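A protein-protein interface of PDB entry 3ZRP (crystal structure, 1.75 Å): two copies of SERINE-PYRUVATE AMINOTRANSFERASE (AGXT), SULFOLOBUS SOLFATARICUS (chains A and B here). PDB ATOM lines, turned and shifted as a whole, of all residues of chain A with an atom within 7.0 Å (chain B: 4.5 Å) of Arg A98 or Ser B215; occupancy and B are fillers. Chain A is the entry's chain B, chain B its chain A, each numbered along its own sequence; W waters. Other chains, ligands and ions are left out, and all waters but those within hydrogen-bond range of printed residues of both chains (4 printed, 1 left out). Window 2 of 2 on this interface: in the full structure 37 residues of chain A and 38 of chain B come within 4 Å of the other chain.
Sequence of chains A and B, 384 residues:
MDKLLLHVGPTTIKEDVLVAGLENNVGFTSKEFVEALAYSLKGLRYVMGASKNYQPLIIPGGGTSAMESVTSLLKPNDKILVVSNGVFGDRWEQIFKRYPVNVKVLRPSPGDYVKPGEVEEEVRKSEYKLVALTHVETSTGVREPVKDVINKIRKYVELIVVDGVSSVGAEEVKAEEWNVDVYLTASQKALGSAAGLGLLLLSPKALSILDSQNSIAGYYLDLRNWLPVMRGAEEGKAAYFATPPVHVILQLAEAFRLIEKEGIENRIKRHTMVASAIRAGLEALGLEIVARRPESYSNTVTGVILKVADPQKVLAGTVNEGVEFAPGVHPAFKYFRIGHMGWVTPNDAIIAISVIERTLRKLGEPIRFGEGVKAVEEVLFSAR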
ATOM      1  N   GLU A  68     -21.320  -9.292  -8.460  1.00  0.00           N
ATOM      2  CA  GLU A  68     -21.320  -9.125  -9.915  1.00  0.00           C
ATOM      3  C   GLU A  68     -21.618 -10.429 -10.698  1.00  0.00           C
ATOM      4  O   GLU A  68     -22.293 -10.404 -11.745  1.00  0.00           O
ATOM      5  CB  GLU A  68     -19.999  -8.478 -10.373  1.00  0.00           C
ATOM      6  CG  GLU A  68     -19.926  -8.210 -11.883  1.00  0.00           C
ATOM      7  CD  GLU A  68     -18.825  -7.183 -12.257  1.00  0.00           C
ATOM      8  OE1 GLU A  68     -18.058  -6.780 -11.372  1.00  0.00           O
ATOM      9  OE2 GLU A  68     -18.754  -6.801 -13.443  1.00  0.00           O
ATOM     10  N   GLU A  93     -26.447  -1.302  -7.442  1.00  0.00           N
ATOM     11  CA  GLU A  93     -26.710  -0.324  -8.518  1.00  0.00           C
ATOM     12  C   GLU A  93     -25.449   0.032  -9.313  1.00  0.00           C
ATOM     13  O   GLU A  93     -25.501   0.086 -10.559  1.00  0.00           O
ATOM     14  CB  GLU A  93     -27.372   0.954  -7.976  1.00  0.00           C
ATOM     15  CG  GLU A  93     -27.834   1.905  -9.056  1.00  0.00           C
ATOM     16  CD  GLU A  93     -28.422   3.218  -8.516  1.00  0.00           C
ATOM     17  OE1 GLU A  93     -28.008   3.730  -7.445  1.00  0.00           O
ATOM     18  OE2 GLU A  93     -29.317   3.746  -9.213  1.00  0.00           O
ATOM     19  N   GLN A  94     -24.324   0.264  -8.621  1.00  0.00           N
ATOM     20  CA  GLN A  94     -23.051   0.572  -9.295  1.00  0.00           C
ATOM     21  C   GLN A  94     -22.594  -0.559 -10.229  1.00  0.00           C
ATOM     22  O   GLN A  94     -22.165  -0.300 -11.367  1.00  0.00           O
ATOM     23  CB  GLN A  94     -21.962   0.952  -8.277  1.00  0.00           C
ATOM     24  CG  GLN A  94     -22.280   2.241  -7.541  1.00  0.00           C
ATOM     25  CD  GLN A  94     -22.349   3.397  -8.503  1.00  0.00           C
ATOM     26  OE1 GLN A  94     -21.354   3.715  -9.164  1.00  0.00           O
ATOM     27  NE2 GLN A  94     -23.519   4.027  -8.609  1.00  0.00           N
ATOM     28  N   ILE A  95     -22.716  -1.805  -9.758  1.00  0.00           N
ATOM     29  CA  ILE A  95     -22.412  -2.995 -10.561  1.00  0.00           C
ATOM     30  C   ILE A  95     -23.355  -3.069 -11.786  1.00  0.00           C
ATOM     31  O   ILE A  95     -22.900  -3.199 -12.940  1.00  0.00           O
ATOM     32  CB  ILE A  95     -22.552  -4.309  -9.724  1.00  0.00           C
ATOM     33  CG1 ILE A  95     -21.513  -4.350  -8.584  1.00  0.00           C
ATOM     34  CG2 ILE A  95     -22.443  -5.548 -10.640  1.00  0.00           C
ATOM     35  CD1 ILE A  95     -21.710  -5.487  -7.577  1.00  0.00           C
ATOM     36  N   PHE A  96     -24.655  -2.980 -11.535  1.00  0.00           N
ATOM     37  CA  PHE A  96     -25.633  -3.165 -12.615  1.00  0.00           C
ATOM     38  C   PHE A  96     -25.642  -2.038 -13.653  1.00  0.00           C
ATOM     39  O   PHE A  96     -26.102  -2.261 -14.773  1.00  0.00           O
ATOM     40  CB  PHE A  96     -27.043  -3.433 -12.088  1.00  0.00           C
ATOM     41  CG  PHE A  96     -27.197  -4.736 -11.347  1.00  0.00           C
ATOM     42  CD1 PHE A  96     -26.675  -5.932 -11.856  1.00  0.00           C
ATOM     43  CD2 PHE A  96     -27.893  -4.768 -10.123  1.00  0.00           C
ATOM     44  CE1 PHE A  96     -26.857  -7.149 -11.165  1.00  0.00           C
ATOM     45  CE2 PHE A  96     -28.068  -5.970  -9.417  1.00  0.00           C
ATOM     46  CZ  PHE A  96     -27.546  -7.154  -9.934  1.00  0.00           C
ATOM     47  N   LYS A  97     -25.103  -0.862 -13.297  1.00  0.00           N
ATOM     48  CA  LYS A  97     -24.897   0.236 -14.241  1.00  0.00           C
ATOM     49  C   LYS A  97     -23.971  -0.163 -15.379  1.00  0.00           C
ATOM     50  O   LYS A  97     -24.004   0.458 -16.438  1.00  0.00           O
ATOM     51  CB  LYS A  97     -24.294   1.462 -13.547  1.00  0.00           C
ATOM     52  CG  LYS A  97     -25.300   2.496 -13.022  1.00  0.00           C
ATOM     53  CD  LYS A  97     -24.543   3.737 -12.498  1.00  0.00           C
ATOM     54  CE  LYS A  97     -25.383   4.590 -11.542  1.00  0.00           C
ATOM     55  NZ  LYS A  97     -26.672   5.117 -12.126  1.00  0.00           N
ATOM     56  N   ARG A  98     -23.137  -1.176 -15.152  1.00  0.00           N
ATOM     57  CA  ARG A  98     -22.194  -1.635 -16.170  1.00  0.00           C
ATOM     58  C   ARG A  98     -22.835  -2.607 -17.175  1.00  0.00           C
ATOM     59  O   ARG A  98     -22.188  -3.021 -18.111  1.00  0.00           O
ATOM     60  CB  ARG A  98     -20.977  -2.298 -15.508  1.00  0.00           C
ATOM     61  CG  ARG A  98     -20.166  -1.392 -14.576  1.00  0.00           C
ATOM     62  CD  ARG A  98     -19.832  -0.032 -15.247  1.00  0.00           C
ATOM     63  NE  ARG A  98     -18.913  -0.255 -16.369  1.00  0.00           N
ATOM     64  CZ  ARG A  98     -18.445   0.706 -17.171  1.00  0.00           C
ATOM     65  NH1 ARG A  98     -18.821   1.967 -16.999  1.00  0.00           N
ATOM     66  NH2 ARG A  98     -17.600   0.414 -18.147  1.00  0.00           N
ATOM     67  N   TYR A  99     -24.084  -3.004 -16.934  1.00  0.00           N
ATOM     68  CA  TYR A  99     -24.743  -4.056 -17.703  1.00  0.00           C
ATOM     69  C   TYR A  99     -26.024  -3.540 -18.344  1.00  0.00           C
ATOM     70  O   TYR A  99     -26.639  -2.634 -17.804  1.00  0.00           O
ATOM     71  CB  TYR A  99     -25.060  -5.271 -16.804  1.00  0.00           C
ATOM     72  CG  TYR A  99     -23.782  -5.980 -16.363  1.00  0.00           C
ATOM     73  CD1 TYR A  99     -23.040  -5.506 -15.258  1.00  0.00           C
ATOM     74  CD2 TYR A  99     -23.273  -7.055 -17.108  1.00  0.00           C
ATOM     75  CE1 TYR A  99     -21.819  -6.129 -14.875  1.00  0.00           C
ATOM     76  CE2 TYR A  99     -22.092  -7.700 -16.735  1.00  0.00           C
ATOM     77  CZ  TYR A  99     -21.359  -7.235 -15.628  1.00  0.00           C
ATOM     78  OH  TYR A  99     -20.192  -7.876 -15.308  1.00  0.00           O
ATOM     79  N   PRO A 100     -26.442  -4.145 -19.485  1.00  0.00           N
ATOM     80  CA  PRO A 100     -27.674  -3.759 -20.205  1.00  0.00           C
ATOM     81  C   PRO A 100     -28.946  -4.217 -19.469  1.00  0.00           C
ATOM     82  O   PRO A 100     -29.707  -5.055 -19.977  1.00  0.00           O
ATOM     83  CB  PRO A 100     -27.532  -4.482 -21.553  1.00  0.00           C
ATOM     84  CG  PRO A 100     -26.712  -5.711 -21.226  1.00  0.00           C
ATOM     85  CD  PRO A 100     -25.744  -5.271 -20.143  1.00  0.00           C
ATOM     86  N   VAL A 101     -29.148  -3.674 -18.270  1.00  0.00           N
ATOM     87  CA  VAL A 101     -30.296  -3.995 -17.444  1.00  0.00           C
ATOM     88  C   VAL A 101     -30.975  -2.728 -16.957  1.00  0.00           C
ATOM     89  O   VAL A 101     -30.391  -1.646 -17.010  1.00  0.00           O
ATOM     90  CB  VAL A 101     -29.944  -4.918 -16.232  1.00  0.00           C
ATOM     91  CG1 VAL A 101     -29.613  -6.321 -16.704  1.00  0.00           C
ATOM     92  CG2 VAL A 101     -28.801  -4.327 -15.387  1.00  0.00           C
ATOM     93  N   THR B  71     -10.218  -5.328 -21.246  1.00  0.00           N
ATOM     94  CA  THR B  71     -11.469  -4.690 -21.741  1.00  0.00           C
ATOM     95  C   THR B  71     -11.665  -3.231 -21.251  1.00  0.00           C
ATOM     96  O   THR B  71     -12.468  -2.477 -21.846  1.00  0.00           O
ATOM     97  CB  THR B  71     -12.716  -5.543 -21.429  1.00  0.00           C
ATOM     98  OG1 THR B  71     -12.830  -5.733 -20.008  1.00  0.00           O
ATOM     99  CG2 THR B  71     -12.602  -6.880 -22.161  1.00  0.00           C
ATOM    100  N   SER B  72     -10.930  -2.854 -20.189  1.00  0.00           N
ATOM    101  CA  SER B  72     -10.902  -1.498 -19.629  1.00  0.00           C
ATOM    102  C   SER B  72     -10.371  -0.489 -20.652  1.00  0.00           C
ATOM    103  O   SER B  72     -10.563   0.739 -20.494  1.00  0.00           O
ATOM    104  CB  SER B  72      -9.998  -1.444 -18.384  1.00  0.00           C
ATOM    105  OG  SER B  72     -10.474  -2.289 -17.317  1.00  0.00           O
ATOM    106  N   LEU B  74     -11.008  -0.755 -24.022  1.00  0.00           N
ATOM    107  CA  LEU B  74     -11.757  -1.012 -25.252  1.00  0.00           C
ATOM    108  C   LEU B  74     -13.114  -0.322 -25.304  1.00  0.00           C
ATOM    109  O   LEU B  74     -13.717   0.017 -24.273  1.00  0.00           O
ATOM    110  CB  LEU B  74     -11.915  -2.523 -25.495  1.00  0.00           C
ATOM    111  CG  LEU B  74     -10.602  -3.316 -25.698  1.00  0.00           C
ATOM    112  CD1 LEU B  74     -10.876  -4.794 -25.807  1.00  0.00           C
ATOM    113  CD2 LEU B  74      -9.832  -2.820 -26.927  1.00  0.00           C
ATOM    114  N   GLN B 213     -11.185   8.148 -20.930  1.00  0.00           N
ATOM    115  CA  GLN B 213     -12.232   7.531 -21.732  1.00  0.00           C
ATOM    116  C   GLN B 213     -13.082   6.562 -20.919  1.00  0.00           C
ATOM    117  O   GLN B 213     -12.628   6.055 -19.880  1.00  0.00           O
ATOM    118  CB  GLN B 213     -11.630   6.782 -22.922  1.00  0.00           C
ATOM    119  CG  GLN B 213     -10.577   7.562 -23.720  1.00  0.00           C
ATOM    120  CD  GLN B 213     -10.146   6.825 -24.982  1.00  0.00           C
ATOM    121  OE1 GLN B 213     -10.944   6.129 -25.618  1.00  0.00           O
ATOM    122  NE2 GLN B 213      -8.880   6.976 -25.350  1.00  0.00           N
ATOM    123  N   ASN B 214     -14.307   6.342 -21.403  1.00  0.00           N
ATOM    124  CA  ASN B 214     -15.203   5.285 -20.926  1.00  0.00           C
ATOM    125  C   ASN B 214     -14.745   3.939 -21.508  1.00  0.00           C
ATOM    126  O   ASN B 214     -13.829   3.890 -22.318  1.00  0.00           O
ATOM    127  CB  ASN B 214     -16.642   5.564 -21.374  1.00  0.00           C
ATOM    128  CG  ASN B 214     -17.170   6.923 -20.899  1.00  0.00           C
ATOM    129  OD1 ASN B 214     -17.370   7.148 -19.699  1.00  0.00           O
ATOM    130  ND2 ASN B 214     -17.405   7.834 -21.851  1.00  0.00           N
ATOM    131  N   SER B 215     -15.391   2.833 -21.119  1.00  0.00           N
ATOM    132  CA  SER B 215     -14.967   1.571 -21.694  1.00  0.00           C
ATOM    133  C   SER B 215     -16.087   0.550 -21.607  1.00  0.00           C
ATOM    134  O   SER B 215     -17.117   0.831 -21.023  1.00  0.00           O
ATOM    135  CB  SER B 215     -13.745   1.000 -20.952  1.00  0.00           C
ATOM    136  OG  SER B 215     -14.157   0.309 -19.767  1.00  0.00           O
ATOM    137  N   ILE B 216     -15.845  -0.618 -22.185  1.00  0.00           N
ATOM    138  CA  ILE B 216     -16.829  -1.708 -22.130  1.00  0.00           C
ATOM    139  C   ILE B 216     -16.626  -2.621 -20.919  1.00  0.00           C
ATOM    140  O   ILE B 216     -17.304  -3.670 -20.814  1.00  0.00           O
ATOM    141  CB  ILE B 216     -16.795  -2.562 -23.424  1.00  0.00           C
ATOM    142  CG1 ILE B 216     -15.431  -3.283 -23.587  1.00  0.00           C
ATOM    143  CG2 ILE B 216     -17.149  -1.669 -24.648  1.00  0.00           C
ATOM    144  CD1 ILE B 216     -15.243  -3.964 -24.952  1.00  0.00           C
ATOM    145  N   ALA B 217     -15.714  -2.268 -20.018  1.00  0.00           N
ATOM    146  CA  ALA B 217     -15.456  -3.130 -18.835  1.00  0.00           C
ATOM    147  C   ALA B 217     -16.697  -3.289 -17.940  1.00  0.00           C
ATOM    148  O   ALA B 217     -17.606  -2.447 -17.935  1.00  0.00           O
ATOM    149  CB  ALA B 217     -14.270  -2.600 -18.021  1.00  0.00           C
ATOM    150  N   GLY B 218     -16.725  -4.394 -17.203  1.00  0.00           N
ATOM    151  CA  GLY B 218     -17.636  -4.542 -16.084  1.00  0.00           C
ATOM    152  C   GLY B 218     -17.245  -3.654 -14.917  1.00  0.00           C
ATOM    153  O   GLY B 218     -16.656  -2.576 -15.071  1.00  0.00           O
ATOM    154  N   TYR B 219     -17.597  -4.099 -13.732  1.00  0.00           N
ATOM    155  CA  TYR B 219     -17.316  -3.356 -12.527  1.00  0.00           C
ATOM    156  C   TYR B 219     -16.037  -3.851 -11.831  1.00  0.00           C
ATOM    157  O   TYR B 219     -15.066  -3.110 -11.737  1.00  0.00           O
ATOM    158  CB  TYR B 219     -18.504  -3.459 -11.585  1.00  0.00           C
ATOM    159  CG  TYR B 219     -18.481  -2.474 -10.432  1.00  0.00           C
ATOM    160  CD1 TYR B 219     -18.694  -1.108 -10.647  1.00  0.00           C
ATOM    161  CD2 TYR B 219     -18.218  -2.913  -9.130  1.00  0.00           C
ATOM    162  CE1 TYR B 219     -18.679  -0.205  -9.581  1.00  0.00           C
ATOM    163  CE2 TYR B 219     -18.214  -2.026  -8.057  1.00  0.00           C
ATOM    164  CZ  TYR B 219     -18.443  -0.679  -8.292  1.00  0.00           C
ATOM    165  OH  TYR B 219     -18.432   0.178  -7.233  1.00  0.00           O
ATOM    166  N   ASP B 222     -12.875  -3.490 -14.063  1.00  0.00           N
ATOM    167  CA  ASP B 222     -12.503  -2.202 -14.662  1.00  0.00           C
ATOM    168  C   ASP B 222     -11.290  -1.685 -13.895  1.00  0.00           C
ATOM    169  O   ASP B 222     -11.373  -1.442 -12.680  1.00  0.00           O
ATOM    170  CB  ASP B 222     -13.682  -1.225 -14.616  1.00  0.00           C
ATOM    171  CG  ASP B 222     -13.360   0.145 -15.230  1.00  0.00           C
ATOM    172  OD1 ASP B 222     -12.202   0.402 -15.637  1.00  0.00           O
ATOM    173  OD2 ASP B 222     -14.292   0.972 -15.274  1.00  0.00           O
ATOM    174  N   ARG B 224      -9.965   1.104 -13.933  1.00  0.00           N
ATOM    175  CA  ARG B 224     -10.277   2.407 -13.312  1.00  0.00           C
ATOM    176  C   ARG B 224     -10.636   2.313 -11.831  1.00  0.00           C
ATOM    177  O   ARG B 224     -10.332   3.214 -11.061  1.00  0.00           O
ATOM    178  CB  ARG B 224     -11.376   3.158 -14.075  1.00  0.00           C
ATOM    179  CG  ARG B 224     -11.007   3.514 -15.494  1.00  0.00           C
ATOM    180  CD  ARG B 224     -12.222   3.958 -16.311  1.00  0.00           C
ATOM    181  NE  ARG B 224     -11.832   4.158 -17.706  1.00  0.00           N
ATOM    182  CZ  ARG B 224     -11.558   3.181 -18.558  1.00  0.00           C
ATOM    183  NH1 ARG B 224     -11.659   1.896 -18.182  1.00  0.00           N
ATOM    184  NH2 ARG B 224     -11.203   3.477 -19.795  1.00  0.00           N
HETATM  185  O   HOH W   1     -15.907  -6.903 -14.198  1.00  0.00           O
HETATM  186  O   HOH W   2     -17.395   3.665 -18.849  1.00  0.00           O
HETATM  187  O   HOH W   3     -16.681   0.107 -14.123  1.00  0.00           O
HETATM  188  O   HOH W   4     -14.805   2.101 -17.773  1.00  0.00           O
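Water W4 lies within hydrogen-bond range of OG of Ser B215 (2.8 Å), OD2 of Asp B222 (2.8 Å), NH1 of Arg B224 (3.2 Å) and NH2 of Arg A98 (3.3 Å). Water W3 lies within hydrogen-bond range of the side-chain carboxylate (OD2) of Asp B222 (2.8 Å), the backbone carbonyl oxygen (O) of Gly B218 (2.8 Å) and the guanidinium group (NE) of Arg A98 (3.2 Å). Water W2 lies within hydrogen-bond range of NH1 of Arg A98 (2.9 Å) and N of Ser B215 (3.1 Å). Water W1 lies within hydrogen-bond range of OE2 of Glu A68 (2.9 Å) and N of Tyr B219 (3.3 Å).
Printed residues of chain B that touch a printed residue of chain A: Ser B215, Ala B217, Gly B218 and Tyr B219. Printed residues of chain A that touch a printed residue of chain B: Glu A68, Gln A94, Ile A95 and Arg A98. Hydrophobic or aromatic side chains of chain A within 4 Å of the printed part of chain B: Ile A95.
No position is printed for both chains. Of the 8 pairs that touch across the chains among the printed residues, none has its exchanged pair printed and touching as well.
The backbone NH of Ala B217 sits at hydrogen-bond distance from the side-chain hydroxyl of Ser B215 (3.0 Å). NH1 of Arg B224 is in hydrogen-bond range of OG of Ser B215, at 3.4 Å. The side-chain hydroxyl (OH) of Tyr A99 lies within hydrogen-bond range of the side-chain carboxylate (OE2) of Glu A68.
Of chain B, only Ser B215 (2.9 Å), Ala B217 (2.9 Å), Gly B218 (3.5 Å) and Tyr B219 (3.8 Å) come within 4 Å of Arg A98. Ser B215 touches just one residue of chain A: Arg A98 (2.9 Å). Of the printed residues of chain B, Ile A95 touches Tyr B219. Printed residues of chain A within 4 Å of Tyr B219: Glu A68 (3.0 Å), Gln A94 (3.6 Å), Ile A95 (3.6 Å) and Arg A98 (3.8 Å). Of the printed residues of chain A, Ala B217 touches Arg A98 (2.9 Å). Of the printed residues of chain A, Gly B218 touches Glu A68 (3.7 Å) and Arg A98 (3.5 Å). Ser B72 touches none of the printed residues of chain A. Leu B74 touches none of the printed residues of chain A. The nearest printed residue of chain A that does not touch Gly B218 is Tyr A99 (4.3 Å).
NH2 of Arg A98 is in hydrogen-bond range of O of Ser B215 (2.9 Å). The guanidinium group (NH2) of Arg A98 lies within hydrogen-bond range of the backbone carbonyl oxygen (O) of Ala B217 (2.9 Å). O of Gly B218 is in hydrogen-bond range of NE of Arg A98 (3.5 Å). The side-chain carboxylate (OE2) of Glu A68 sits at hydrogen-bond distance from the backbone NH (N) of Tyr B219, 3.0 Å away.
Among the printed residues, merely in contact across the chains: Glu A68 with Gly B218 (3.7 Å), Gln A94 with Tyr B219 (3.6 Å), Ile A95 with Tyr B219 (3.6 Å) and Arg A98 with Tyr B219 (3.8 Å).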
